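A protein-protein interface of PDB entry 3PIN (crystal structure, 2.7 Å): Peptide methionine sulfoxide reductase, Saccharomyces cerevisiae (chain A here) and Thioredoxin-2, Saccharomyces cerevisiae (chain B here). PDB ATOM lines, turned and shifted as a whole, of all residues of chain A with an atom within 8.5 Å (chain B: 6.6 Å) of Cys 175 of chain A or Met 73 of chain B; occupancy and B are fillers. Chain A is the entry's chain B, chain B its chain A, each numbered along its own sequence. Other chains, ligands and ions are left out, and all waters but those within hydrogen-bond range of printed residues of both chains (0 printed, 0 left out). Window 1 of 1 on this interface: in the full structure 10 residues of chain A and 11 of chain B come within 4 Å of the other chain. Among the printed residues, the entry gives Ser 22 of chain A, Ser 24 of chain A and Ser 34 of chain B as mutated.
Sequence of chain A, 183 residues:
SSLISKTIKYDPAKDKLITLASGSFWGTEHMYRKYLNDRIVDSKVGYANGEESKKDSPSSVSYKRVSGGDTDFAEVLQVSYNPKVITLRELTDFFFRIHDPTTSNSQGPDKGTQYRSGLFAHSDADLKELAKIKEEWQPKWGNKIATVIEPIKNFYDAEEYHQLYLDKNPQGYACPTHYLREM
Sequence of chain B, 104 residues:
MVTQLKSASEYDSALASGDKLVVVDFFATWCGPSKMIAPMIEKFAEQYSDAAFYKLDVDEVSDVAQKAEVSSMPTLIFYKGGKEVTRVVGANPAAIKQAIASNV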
ATOM      1  N   SER A  22       5.533 -13.228 -10.641  1.00  0.00           N
ATOM      2  CA  SER A  22       4.417 -13.902 -11.291  1.00  0.00           C
ATOM      3  C   SER A  22       4.251 -13.469 -12.748  1.00  0.00           C
ATOM      4  O   SER A  22       3.239 -13.775 -13.379  1.00  0.00           O
ATOM      5  CB  SER A  22       3.121 -13.698 -10.500  1.00  0.00           C
ATOM      6  OG  SER A  22       2.744 -12.335 -10.466  1.00  0.00           O
ATOM      7  N   GLY A  23       5.251 -12.766 -13.275  1.00  0.00           N
ATOM      8  CA  GLY A  23       5.283 -12.408 -14.694  1.00  0.00           C
ATOM      9  C   GLY A  23       5.080 -10.936 -14.988  1.00  0.00           C
ATOM     10  O   GLY A  23       5.347 -10.480 -16.099  1.00  0.00           O
ATOM     11  N   SER A  24       4.599 -10.203 -13.990  1.00  0.00           N
ATOM     12  CA  SER A  24       4.369  -8.770 -14.078  1.00  0.00           C
ATOM     13  C   SER A  24       4.144  -8.254 -12.674  1.00  0.00           C
ATOM     14  O   SER A  24       3.244  -8.740 -11.981  1.00  0.00           O
ATOM     15  CB  SER A  24       3.124  -8.485 -14.919  1.00  0.00           C
ATOM     16  OG  SER A  24       2.566  -7.215 -14.619  1.00  0.00           O
ATOM     17  N   PHE A  25       4.941  -7.273 -12.247  1.00  0.00           N
ATOM     18  CA  PHE A  25       4.730  -6.697 -10.916  1.00  0.00           C
ATOM     19  C   PHE A  25       3.438  -5.871 -10.797  1.00  0.00           C
ATOM     20  O   PHE A  25       2.995  -5.570  -9.690  1.00  0.00           O
ATOM     21  CB  PHE A  25       5.973  -5.971 -10.345  1.00  0.00           C
ATOM     22  CG  PHE A  25       6.557  -4.894 -11.231  1.00  0.00           C
ATOM     23  CD1 PHE A  25       7.938  -4.720 -11.279  1.00  0.00           C
ATOM     24  CD2 PHE A  25       5.751  -4.036 -11.981  1.00  0.00           C
ATOM     25  CE1 PHE A  25       8.514  -3.728 -12.072  1.00  0.00           C
ATOM     26  CE2 PHE A  25       6.321  -3.040 -12.783  1.00  0.00           C
ATOM     27  CZ  PHE A  25       7.705  -2.888 -12.826  1.00  0.00           C
ATOM     28  N   TRP A  26       2.830  -5.524 -11.930  1.00  0.00           N
ATOM     29  CA  TRP A  26       1.525  -4.868 -11.920  1.00  0.00           C
ATOM     30  C   TRP A  26       0.485  -5.844 -11.396  1.00  0.00           C
ATOM     31  O   TRP A  26      -0.366  -5.482 -10.581  1.00  0.00           O
ATOM     32  CB  TRP A  26       1.150  -4.365 -13.315  1.00  0.00           C
ATOM     33  CG  TRP A  26       2.177  -3.446 -13.863  1.00  0.00           C
ATOM     34  CD1 TRP A  26       3.131  -3.745 -14.788  1.00  0.00           C
ATOM     35  CD2 TRP A  26       2.385  -2.083 -13.493  1.00  0.00           C
ATOM     36  NE1 TRP A  26       3.914  -2.647 -15.030  1.00  0.00           N
ATOM     37  CE2 TRP A  26       3.481  -1.612 -14.245  1.00  0.00           C
ATOM     38  CE3 TRP A  26       1.748  -1.208 -12.605  1.00  0.00           C
ATOM     39  CZ2 TRP A  26       3.953  -0.304 -14.138  1.00  0.00           C
ATOM     40  CZ3 TRP A  26       2.218   0.094 -12.499  1.00  0.00           C
ATOM     41  CH2 TRP A  26       3.311   0.532 -13.262  1.00  0.00           C
ATOM     42  N   GLY A  27       0.589  -7.089 -11.853  1.00  0.00           N
ATOM     43  CA  GLY A  27      -0.270  -8.165 -11.389  1.00  0.00           C
ATOM     44  C   GLY A  27       0.041  -8.602  -9.975  1.00  0.00           C
ATOM     45  O   GLY A  27      -0.871  -8.829  -9.182  1.00  0.00           O
ATOM     46  N   THR A  28       1.327  -8.721  -9.652  1.00  0.00           N
ATOM     47  CA  THR A  28       1.733  -9.194  -8.330  1.00  0.00           C
ATOM     48  C   THR A  28       1.293  -8.207  -7.248  1.00  0.00           C
ATOM     49  O   THR A  28       0.750  -8.613  -6.219  1.00  0.00           O
ATOM     50  CB  THR A  28       3.260  -9.480  -8.236  1.00  0.00           C
ATOM     51  OG1 THR A  28       3.682 -10.231  -9.378  1.00  0.00           O
ATOM     52  CG2 THR A  28       3.573 -10.302  -7.004  1.00  0.00           C
ATOM     53  N   GLU A  75      10.621  -8.965 -12.968  1.00  0.00           N
ATOM     54  CA  GLU A  75       9.697  -8.019 -12.351  1.00  0.00           C
ATOM     55  C   GLU A  75       9.069  -8.698 -11.143  1.00  0.00           C
ATOM     56  O   GLU A  75       8.463  -9.763 -11.269  1.00  0.00           O
ATOM     57  CB  GLU A  75       8.616  -7.580 -13.341  1.00  0.00           C
ATOM     58  CG  GLU A  75       9.048  -6.491 -14.314  1.00  0.00           C
ATOM     59  CD  GLU A  75       7.877  -5.854 -15.071  1.00  0.00           C
ATOM     60  OE1 GLU A  75       6.704  -6.199 -14.793  1.00  0.00           O
ATOM     61  OE2 GLU A  75       8.134  -4.999 -15.952  1.00  0.00           O
ATOM     62  N   GLN A 171       7.115  -9.702 -20.793  1.00  0.00           N
ATOM     63  CA  GLN A 171       8.349  -9.078 -20.331  1.00  0.00           C
ATOM     64  C   GLN A 171       7.968  -7.823 -19.528  1.00  0.00           C
ATOM     65  O   GLN A 171       7.449  -7.927 -18.406  1.00  0.00           O
ATOM     66  CB  GLN A 171       9.240  -8.752 -21.538  1.00  0.00           C
ATOM     67  CG  GLN A 171      10.724  -9.039 -21.344  1.00  0.00           C
ATOM     68  CD  GLN A 171      11.512  -7.825 -20.869  1.00  0.00           C
ATOM     69  OE1 GLN A 171      11.491  -6.764 -21.507  1.00  0.00           O
ATOM     70  NE2 GLN A 171      12.227  -7.982 -19.753  1.00  0.00           N
ATOM     71  N   GLY A 172       8.227  -6.648 -20.102  1.00  0.00           N
ATOM     72  CA  GLY A 172       7.628  -5.397 -19.640  1.00  0.00           C
ATOM     73  C   GLY A 172       6.701  -4.907 -20.741  1.00  0.00           C
ATOM     74  O   GLY A 172       6.325  -3.732 -20.793  1.00  0.00           O
ATOM     75  N   TYR A 173       6.352  -5.833 -21.634  1.00  0.00           N
ATOM     76  CA  TYR A 173       5.457  -5.574 -22.750  1.00  0.00           C
ATOM     77  C   TYR A 173       4.029  -5.964 -22.415  1.00  0.00           C
ATOM     78  O   TYR A 173       3.086  -5.393 -22.950  1.00  0.00           O
ATOM     79  CB  TYR A 173       5.907  -6.360 -23.984  1.00  0.00           C
ATOM     80  CG  TYR A 173       6.938  -5.657 -24.829  1.00  0.00           C
ATOM     81  CD1 TYR A 173       8.292  -5.967 -24.710  1.00  0.00           C
ATOM     82  CD2 TYR A 173       6.560  -4.682 -25.751  1.00  0.00           C
ATOM     83  CE1 TYR A 173       9.248  -5.320 -25.493  1.00  0.00           C
ATOM     84  CE2 TYR A 173       7.504  -4.030 -26.537  1.00  0.00           C
ATOM     85  CZ  TYR A 173       8.844  -4.354 -26.405  1.00  0.00           C
ATOM     86  OH  TYR A 173       9.778  -3.708 -27.183  1.00  0.00           O
ATOM     87  N   ALA A 174       3.879  -6.950 -21.535  1.00  0.00           N
ATOM     88  CA  ALA A 174       2.570  -7.502 -21.211  1.00  0.00           C
ATOM     89  C   ALA A 174       2.498  -8.039 -19.785  1.00  0.00           C
ATOM     90  O   ALA A 174       3.509  -8.473 -19.228  1.00  0.00           O
ATOM     91  CB  ALA A 174       2.201  -8.598 -22.208  1.00  0.00           C
ATOM     92  N   CYS A 175       1.302  -7.992 -19.198  1.00  0.00           N
ATOM     93  CA  CYS A 175       1.034  -8.668 -17.928  1.00  0.00           C
ATOM     94  C   CYS A 175       0.269  -9.954 -18.204  1.00  0.00           C
ATOM     95  O   CYS A 175      -0.731  -9.924 -18.927  1.00  0.00           O
ATOM     96  CB  CYS A 175       0.196  -7.799 -16.987  1.00  0.00           C
ATOM     97  SG  CYS A 175       0.667  -6.073 -16.857  1.00  0.00           S
ATOM     98  N   PRO A 176       0.747 -11.092 -17.661  1.00  0.00           N
ATOM     99  CA  PRO A 176      -0.078 -12.304 -17.706  1.00  0.00           C
ATOM    100  C   PRO A 176      -1.353 -12.121 -16.893  1.00  0.00           C
ATOM    101  O   PRO A 176      -1.407 -11.246 -16.028  1.00  0.00           O
ATOM    102  CB  PRO A 176       0.810 -13.384 -17.077  1.00  0.00           C
ATOM    103  CG  PRO A 176       2.075 -12.729 -16.690  1.00  0.00           C
ATOM    104  CD  PRO A 176       2.147 -11.381 -17.312  1.00  0.00           C
ATOM    105  N   THR A 177      -2.375 -12.923 -17.184  1.00  0.00           N
ATOM    106  CA  THR A 177      -3.647 -12.816 -16.469  1.00  0.00           C
ATOM    107  C   THR A 177      -3.471 -13.088 -14.976  1.00  0.00           C
ATOM    108  O   THR A 177      -2.980 -14.145 -14.573  1.00  0.00           O
ATOM    109  CB  THR A 177      -4.748 -13.725 -17.061  1.00  0.00           C
ATOM    110  OG1 THR A 177      -4.257 -15.062 -17.188  1.00  0.00           O
ATOM    111  CG2 THR A 177      -5.184 -13.226 -18.430  1.00  0.00           C
ATOM    112  N   HIS A 178      -3.851 -12.102 -14.172  1.00  0.00           N
ATOM    113  CA  HIS A 178      -3.844 -12.218 -12.720  1.00  0.00           C
ATOM    114  C   HIS A 178      -5.270 -12.155 -12.169  1.00  0.00           C
ATOM    115  O   HIS A 178      -5.985 -11.172 -12.371  1.00  0.00           O
ATOM    116  CB  HIS A 178      -2.971 -11.125 -12.093  1.00  0.00           C
ATOM    117  CG  HIS A 178      -1.503 -11.420 -12.143  1.00  0.00           C
ATOM    118  ND1 HIS A 178      -0.790 -11.461 -13.326  1.00  0.00           N
ATOM    119  CD2 HIS A 178      -0.614 -11.687 -11.156  1.00  0.00           C
ATOM    120  CE1 HIS A 178       0.473 -11.745 -13.064  1.00  0.00           C
ATOM    121  NE2 HIS A 178       0.606 -11.884 -11.755  1.00  0.00           N
ATOM    122  N   TYR A 179      -5.673 -13.232 -11.500  1.00  0.00           N
ATOM    123  CA  TYR A 179      -6.953 -13.324 -10.790  1.00  0.00           C
ATOM    124  C   TYR A 179      -6.938 -14.563  -9.894  1.00  0.00           C
ATOM    125  O   TYR A 179      -6.163 -15.500 -10.127  1.00  0.00           O
ATOM    126  CB  TYR A 179      -8.140 -13.378 -11.764  1.00  0.00           C
ATOM    127  CG  TYR A 179      -8.217 -14.636 -12.606  1.00  0.00           C
ATOM    128  CD1 TYR A 179      -8.916 -15.759 -12.153  1.00  0.00           C
ATOM    129  CD2 TYR A 179      -7.604 -14.699 -13.861  1.00  0.00           C
ATOM    130  CE1 TYR A 179      -8.994 -16.915 -12.921  1.00  0.00           C
ATOM    131  CE2 TYR A 179      -7.676 -15.851 -14.638  1.00  0.00           C
ATOM    132  CZ  TYR A 179      -8.371 -16.953 -14.160  1.00  0.00           C
ATOM    133  OH  TYR A 179      -8.454 -18.094 -14.920  1.00  0.00           O
ATOM    134  N   ASP B  25      -8.972  -4.573 -28.473  1.00  0.00           N
ATOM    135  CA  ASP B  25      -7.931  -4.456 -27.445  1.00  0.00           C
ATOM    136  C   ASP B  25      -8.397  -5.126 -26.151  1.00  0.00           C
ATOM    137  O   ASP B  25      -9.258  -4.602 -25.440  1.00  0.00           O
ATOM    138  CB  ASP B  25      -7.586  -2.976 -27.204  1.00  0.00           C
ATOM    139  CG  ASP B  25      -6.570  -2.763 -26.070  1.00  0.00           C
ATOM    140  OD1 ASP B  25      -5.964  -3.740 -25.568  1.00  0.00           O
ATOM    141  OD2 ASP B  25      -6.372  -1.591 -25.680  1.00  0.00           O
ATOM    142  N   PHE B  26      -7.834  -6.291 -25.856  1.00  0.00           N
ATOM    143  CA  PHE B  26      -8.126  -6.978 -24.602  1.00  0.00           C
ATOM    144  C   PHE B  26      -7.211  -6.422 -23.515  1.00  0.00           C
ATOM    145  O   PHE B  26      -5.993  -6.587 -23.585  1.00  0.00           O
ATOM    146  CB  PHE B  26      -7.934  -8.490 -24.757  1.00  0.00           C
ATOM    147  CG  PHE B  26      -9.011  -9.161 -25.560  1.00  0.00           C
ATOM    148  CD1 PHE B  26      -8.954  -9.187 -26.950  1.00  0.00           C
ATOM    149  CD2 PHE B  26     -10.082  -9.776 -24.927  1.00  0.00           C
ATOM    150  CE1 PHE B  26      -9.954  -9.810 -27.695  1.00  0.00           C
ATOM    151  CE2 PHE B  26     -11.081 -10.405 -25.664  1.00  0.00           C
ATOM    152  CZ  PHE B  26     -11.017 -10.422 -27.050  1.00  0.00           C
ATOM    153  N   PHE B  27      -7.799  -5.767 -22.516  1.00  0.00           N
ATOM    154  CA  PHE B  27      -7.011  -4.999 -21.552  1.00  0.00           C
ATOM    155  C   PHE B  27      -7.322  -5.274 -20.082  1.00  0.00           C
ATOM    156  O   PHE B  27      -8.354  -5.855 -19.746  1.00  0.00           O
ATOM    157  CB  PHE B  27      -7.133  -3.492 -21.840  1.00  0.00           C
ATOM    158  CG  PHE B  27      -8.449  -2.886 -21.423  1.00  0.00           C
ATOM    159  CD1 PHE B  27      -8.608  -2.336 -20.151  1.00  0.00           C
ATOM    160  CD2 PHE B  27      -9.520  -2.841 -22.307  1.00  0.00           C
ATOM    161  CE1 PHE B  27      -9.822  -1.764 -19.761  1.00  0.00           C
ATOM    162  CE2 PHE B  27     -10.732  -2.275 -21.927  1.00  0.00           C
ATOM    163  CZ  PHE B  27     -10.883  -1.735 -20.651  1.00  0.00           C
ATOM    164  N   ALA B  28      -6.405  -4.836 -19.222  1.00  0.00           N
ATOM    165  CA  ALA B  28      -6.578  -4.873 -17.779  1.00  0.00           C
ATOM    166  C   ALA B  28      -6.244  -3.499 -17.211  1.00  0.00           C
ATOM    167  O   ALA B  28      -5.241  -2.891 -17.586  1.00  0.00           O
ATOM    168  CB  ALA B  28      -5.688  -5.935 -17.169  1.00  0.00           C
ATOM    169  N   TRP B  30      -5.321  -2.690 -14.260  1.00  0.00           N
ATOM    170  CA  TRP B  30      -4.197  -2.729 -13.330  1.00  0.00           C
ATOM    171  C   TRP B  30      -2.871  -2.873 -14.066  1.00  0.00           C
ATOM    172  O   TRP B  30      -1.817  -2.545 -13.522  1.00  0.00           O
ATOM    173  CB  TRP B  30      -4.367  -3.866 -12.318  1.00  0.00           C
ATOM    174  CG  TRP B  30      -4.827  -5.153 -12.930  1.00  0.00           C
ATOM    175  CD1 TRP B  30      -6.115  -5.591 -13.038  1.00  0.00           C
ATOM    176  CD2 TRP B  30      -4.006  -6.166 -13.528  1.00  0.00           C
ATOM    177  NE1 TRP B  30      -6.149  -6.815 -13.661  1.00  0.00           N
ATOM    178  CE2 TRP B  30      -4.870  -7.191 -13.974  1.00  0.00           C
ATOM    179  CE3 TRP B  30      -2.628  -6.310 -13.727  1.00  0.00           C
ATOM    180  CZ2 TRP B  30      -4.399  -8.343 -14.609  1.00  0.00           C
ATOM    181  CZ3 TRP B  30      -2.162  -7.453 -14.360  1.00  0.00           C
ATOM    182  CH2 TRP B  30      -3.046  -8.457 -14.790  1.00  0.00           C
ATOM    183  N   CYS B  31      -2.938  -3.361 -15.303  1.00  0.00           N
ATOM    184  CA  CYS B  31      -1.746  -3.655 -16.091  1.00  0.00           C
ATOM    185  C   CYS B  31      -1.172  -2.403 -16.742  1.00  0.00           C
ATOM    186  O   CYS B  31      -1.829  -1.765 -17.568  1.00  0.00           O
ATOM    187  CB  CYS B  31      -2.042  -4.730 -17.140  1.00  0.00           C
ATOM    188  SG  CYS B  31      -0.617  -5.173 -18.158  1.00  0.00           S
ATOM    189  N   GLY B  32       0.060  -2.068 -16.357  1.00  0.00           N
ATOM    190  CA  GLY B  32       0.778  -0.897 -16.868  1.00  0.00           C
ATOM    191  C   GLY B  32       0.898  -0.837 -18.384  1.00  0.00           C
ATOM    192  O   GLY B  32       0.414   0.115 -18.998  1.00  0.00           O
ATOM    193  N   PRO B  33       1.553  -1.845 -18.996  1.00  0.00           N
ATOM    194  CA  PRO B  33       1.653  -1.948 -20.451  1.00  0.00           C
ATOM    195  C   PRO B  33       0.301  -1.820 -21.154  1.00  0.00           C
ATOM    196  O   PRO B  33       0.171  -1.046 -22.107  1.00  0.00           O
ATOM    197  CB  PRO B  33       2.217  -3.354 -20.654  1.00  0.00           C
ATOM    198  CG  PRO B  33       3.054  -3.578 -19.471  1.00  0.00           C
ATOM    199  CD  PRO B  33       2.365  -2.880 -18.329  1.00  0.00           C
ATOM    200  N   SER B  34      -0.692  -2.567 -20.674  1.00  0.00           N
ATOM    201  CA  SER B  34      -2.042  -2.545 -21.234  1.00  0.00           C
ATOM    202  C   SER B  34      -2.656  -1.150 -21.186  1.00  0.00           C
ATOM    203  O   SER B  34      -3.333  -0.728 -22.120  1.00  0.00           O
ATOM    204  CB  SER B  34      -2.931  -3.535 -20.480  1.00  0.00           C
ATOM    205  OG  SER B  34      -4.302  -3.279 -20.700  1.00  0.00           O
ATOM    206  N   LEU B  56     -11.953  -4.412 -24.605  1.00  0.00           N
ATOM    207  CA  LEU B  56     -12.633  -5.321 -23.697  1.00  0.00           C
ATOM    208  C   LEU B  56     -11.808  -5.541 -22.433  1.00  0.00           C
ATOM    209  O   LEU B  56     -10.638  -5.920 -22.502  1.00  0.00           O
ATOM    210  CB  LEU B  56     -12.918  -6.652 -24.399  1.00  0.00           C
ATOM    211  CG  LEU B  56     -13.745  -7.706 -23.654  1.00  0.00           C
ATOM    212  CD1 LEU B  56     -14.670  -8.447 -24.608  1.00  0.00           C
ATOM    213  CD2 LEU B  56     -12.858  -8.685 -22.876  1.00  0.00           C
ATOM    214  N   VAL B  58     -10.723  -7.623 -19.476  1.00  0.00           N
ATOM    215  CA  VAL B  58     -10.624  -9.064 -19.239  1.00  0.00           C
ATOM    216  C   VAL B  58     -11.169  -9.480 -17.869  1.00  0.00           C
ATOM    217  O   VAL B  58     -11.592 -10.622 -17.685  1.00  0.00           O
ATOM    218  CB  VAL B  58      -9.178  -9.593 -19.451  1.00  0.00           C
ATOM    219  CG1 VAL B  58      -8.755  -9.429 -20.909  1.00  0.00           C
ATOM    220  CG2 VAL B  58      -8.183  -8.894 -18.521  1.00  0.00           C
ATOM    221  N   ASP B  59     -11.165  -8.551 -16.917  1.00  0.00           N
ATOM    222  CA  ASP B  59     -11.762  -8.794 -15.610  1.00  0.00           C
ATOM    223  C   ASP B  59     -13.282  -8.682 -15.698  1.00  0.00           C
ATOM    224  O   ASP B  59     -14.007  -9.483 -15.092  1.00  0.00           O
ATOM    225  CB  ASP B  59     -11.199  -7.825 -14.563  1.00  0.00           C
ATOM    226  CG  ASP B  59      -9.687  -7.964 -14.379  1.00  0.00           C
ATOM    227  OD1 ASP B  59      -9.140  -9.076 -14.582  1.00  0.00           O
ATOM    228  OD2 ASP B  59      -9.044  -6.954 -14.021  1.00  0.00           O
ATOM    229  N   VAL B  70      -6.898 -15.275 -24.463  1.00  0.00           N
ATOM    230  CA  VAL B  70      -6.027 -14.177 -24.092  1.00  0.00           C
ATOM    231  C   VAL B  70      -5.463 -14.479 -22.708  1.00  0.00           C
ATOM    232  O   VAL B  70      -6.212 -14.629 -21.740  1.00  0.00           O
ATOM    233  CB  VAL B  70      -6.798 -12.831 -24.087  1.00  0.00           C
ATOM    234  CG1 VAL B  70      -5.947 -11.714 -23.502  1.00  0.00           C
ATOM    235  CG2 VAL B  70      -7.255 -12.476 -25.510  1.00  0.00           C
ATOM    236  N   SER B  71      -4.137 -14.583 -22.635  1.00  0.00           N
ATOM    237  CA  SER B  71      -3.432 -14.869 -21.390  1.00  0.00           C
ATOM    238  C   SER B  71      -2.436 -13.762 -21.012  1.00  0.00           C
ATOM    239  O   SER B  71      -1.667 -13.904 -20.062  1.00  0.00           O
ATOM    240  CB  SER B  71      -2.731 -16.227 -21.489  1.00  0.00           C
ATOM    241  OG  SER B  71      -1.963 -16.318 -22.676  1.00  0.00           O
ATOM    242  N   SER B  72      -2.462 -12.660 -21.758  1.00  0.00           N
ATOM    243  CA  SER B  72      -1.613 -11.501 -21.489  1.00  0.00           C
ATOM    244  C   SER B  72      -2.260 -10.232 -22.007  1.00  0.00           C
ATOM    245  O   SER B  72      -3.027 -10.266 -22.964  1.00  0.00           O
ATOM    246  CB  SER B  72      -0.242 -11.658 -22.144  1.00  0.00           C
ATOM    247  OG  SER B  72       0.550 -12.569 -21.419  1.00  0.00           O
ATOM    248  N   MET B  73      -1.944  -9.110 -21.369  1.00  0.00           N
ATOM    249  CA  MET B  73      -2.486  -7.820 -21.782  1.00  0.00           C
ATOM    250  C   MET B  73      -1.358  -6.820 -21.982  1.00  0.00           C
ATOM    251  O   MET B  73      -0.467  -6.728 -21.144  1.00  0.00           O
ATOM    252  CB  MET B  73      -3.507  -7.294 -20.768  1.00  0.00           C
ATOM    253  CG  MET B  73      -4.793  -8.110 -20.672  1.00  0.00           C
ATOM    254  SD  MET B  73      -4.575  -9.723 -19.886  1.00  0.00           S
ATOM    255  CE  MET B  73      -4.020  -9.258 -18.242  1.00  0.00           C
ATOM    256  N   PRO B  74      -1.403  -6.059 -23.093  1.00  0.00           N
ATOM    257  CA  PRO B  74      -2.505  -6.080 -24.050  1.00  0.00           C
ATOM    258  C   PRO B  74      -2.399  -7.206 -25.075  1.00  0.00           C
ATOM    259  O   PRO B  74      -1.300  -7.664 -25.404  1.00  0.00           O
ATOM    260  CB  PRO B  74      -2.361  -4.733 -24.750  1.00  0.00           C
ATOM    261  CG  PRO B  74      -0.890  -4.498 -24.774  1.00  0.00           C
ATOM    262  CD  PRO B  74      -0.339  -5.125 -23.510  1.00  0.00           C
ATOM    263  N   THR B  75      -3.551  -7.654 -25.557  1.00  0.00           N
ATOM    264  CA  THR B  75      -3.614  -8.506 -26.729  1.00  0.00           C
ATOM    265  C   THR B  75      -4.593  -7.865 -27.692  1.00  0.00           C
ATOM    266  O   THR B  75      -5.779  -7.733 -27.393  1.00  0.00           O
ATOM    267  CB  THR B  75      -4.046  -9.948 -26.392  1.00  0.00           C
ATOM    268  OG1 THR B  75      -3.080 -10.543 -25.518  1.00  0.00           O
ATOM    269  CG2 THR B  75      -4.140 -10.787 -27.661  1.00  0.00           C
ATOM    270  N   VAL B  89       0.582  -9.658 -29.336  1.00  0.00           N
ATOM    271  CA  VAL B  89       0.635  -9.708 -27.877  1.00  0.00           C
ATOM    272  C   VAL B  89       1.728  -8.773 -27.384  1.00  0.00           C
ATOM    273  O   VAL B  89       2.846  -8.784 -27.905  1.00  0.00           O
ATOM    274  CB  VAL B  89       0.871 -11.153 -27.350  1.00  0.00           C
ATOM    275  CG1 VAL B  89       0.768 -11.202 -25.828  1.00  0.00           C
ATOM    276  CG2 VAL B  89      -0.131 -12.132 -27.978  1.00  0.00           C
ATOM    277  N   GLY B  90       1.400  -7.961 -26.383  1.00  0.00           N
ATOM    278  CA  GLY B  90       2.361  -7.022 -25.811  1.00  0.00           C
ATOM    279  C   GLY B  90       2.214  -5.621 -26.372  1.00  0.00           C
ATOM    280  O   GLY B  90       1.665  -5.425 -27.463  1.00  0.00           O
ATOM    281  N   ALA B  91       2.724  -4.645 -25.622  1.00  0.00           N
ATOM    282  CA  ALA B  91       2.593  -3.236 -25.984  1.00  0.00           C
ATOM    283  C   ALA B  91       3.665  -2.749 -26.972  1.00  0.00           C
ATOM    284  O   ALA B  91       4.542  -1.956 -26.615  1.00  0.00           O
ATOM    285  CB  ALA B  91       2.569  -2.366 -24.717  1.00  0.00           C
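Of chain B, only Trp 30, Cys 31, Pro 33, Ser 72 and Met 73 come within 4 Å of Cys 175 of chain A.
Ser 72 of chain B touches three residues of chain A.
Of chain A, only Tyr 173 comes within 4 Å of Pro 74 of chain B.
Printed residues of chain B within 4 Å of Thr 177 of chain A: Val 70 (3.7 Å), Ser 71 (3.1 Å) and Met 73 (3.8 Å).
Of the printed residues of chain B, Pro 176 of chain A touches Trp 30 (3.5 Å), Ser 71 (3.3 Å), Ser 72 (3.8 Å) and Met 73 (3.96 Å).
Of the printed residues of chain B, Ala 174 of chain A touches Ser 72 (3.9 Å), Met 73 (3.1 Å) and Gly 90 (3.9 Å).
The nearest residue of chain B that does not touch Cys 175 of chain A is Gly 32 of chain B (4.1 Å).
The nearest residue of chain A that does not touch Met 73 of chain B is Tyr 173 of chain A (4.2 Å).
The nearest printed residue of chain A that does not touch Cys 31 of chain B is Trp 26 of chain A (4.1 Å).
The indole nitrogen (NE1) of Trp 30 of chain B sits at hydrogen-bond distance from the side-chain carboxylate (OD2) of Asp 59 of chain B, at 2.9 Å.
N of Ser 34 of chain B is in hydrogen-bond range of SG of Cys 31 of chain B, at 3.6 Å.
OG1 of Thr 75 of chain B lies within hydrogen-bond range of O of Ser 72 of chain B (2.6 Å).
The side-chain hydroxyl of Ser 24 of chain A sits close to the backbone NH of Trp 26 of chain A (3.2 Å).
The side-chain hydroxyl of Ser 24 of chain A is in hydrogen-bond range of the backbone NH of Gly 27 of chain A, 3.4 Å away.
The backbone carbonyl oxygen (O) of Pro 176 of chain A is in hydrogen-bond range of a ring nitrogen (ND1) of His 178 of chain A (2.8 Å).
Hydrophobic or aromatic side chains of chain B within 4 Å of the printed part of chain A: Trp 30, Pro 33, Met 73, Pro 74 and Ala 91.
Hydrophobic or aromatic side chains of chain A within 4 Å of the printed part of chain B: Trp 26, Tyr 173, Ala 174, Pro 176 and His 178.
Along chain A the printed residues that touch a printed residue of chain B span positions 26 to 178.
Among the printed residues, no Asp or Glu carboxylate lies within 4 Å of a Lys or Arg side-chain nitrogen of the other chain.
Trp 26 of chain A touches Pro 33 of chain B.
Trp 30 of chain B touches Gly 27 of chain A (CZ3 to CA, 3.6 Å).
Gly 172 of chain A touches Pro 33 of chain B.
Tyr 173 of chain A touches Pro 33 of chain B.
Ser 72 of chain B touches Ala 174 of chain A.
Met 73 of chain B touches Ala 174 of chain A.
Gly 90 of chain B touches Ala 174 of chain A.
Cys 175 of chain A touches Pro 33 of chain B.
CG2 of Thr 177 of chain A touches SD of Met 73 of chain B, 3.8 Å away.
Trp 30 of chain B touches His 178 of chain A (CH2 to N, 3.8 Å).
The side-chain sulfur (SG) of Cys 175 of chain A forms a disulfide with the side-chain sulfur (SG) of Cys 31 of chain B, at 2.0 Å.
N of Thr 177 of chain A lies within hydrogen-bond range of O of Ser 71 of chain B (3.1 Å).
N of Met 73 of chain B lies within hydrogen-bond range of O of Cys 175 of chain A (2.8 Å).
N of Ala 91 of chain B lies within hydrogen-bond range of O of Tyr 173 of chain A (2.8 Å).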
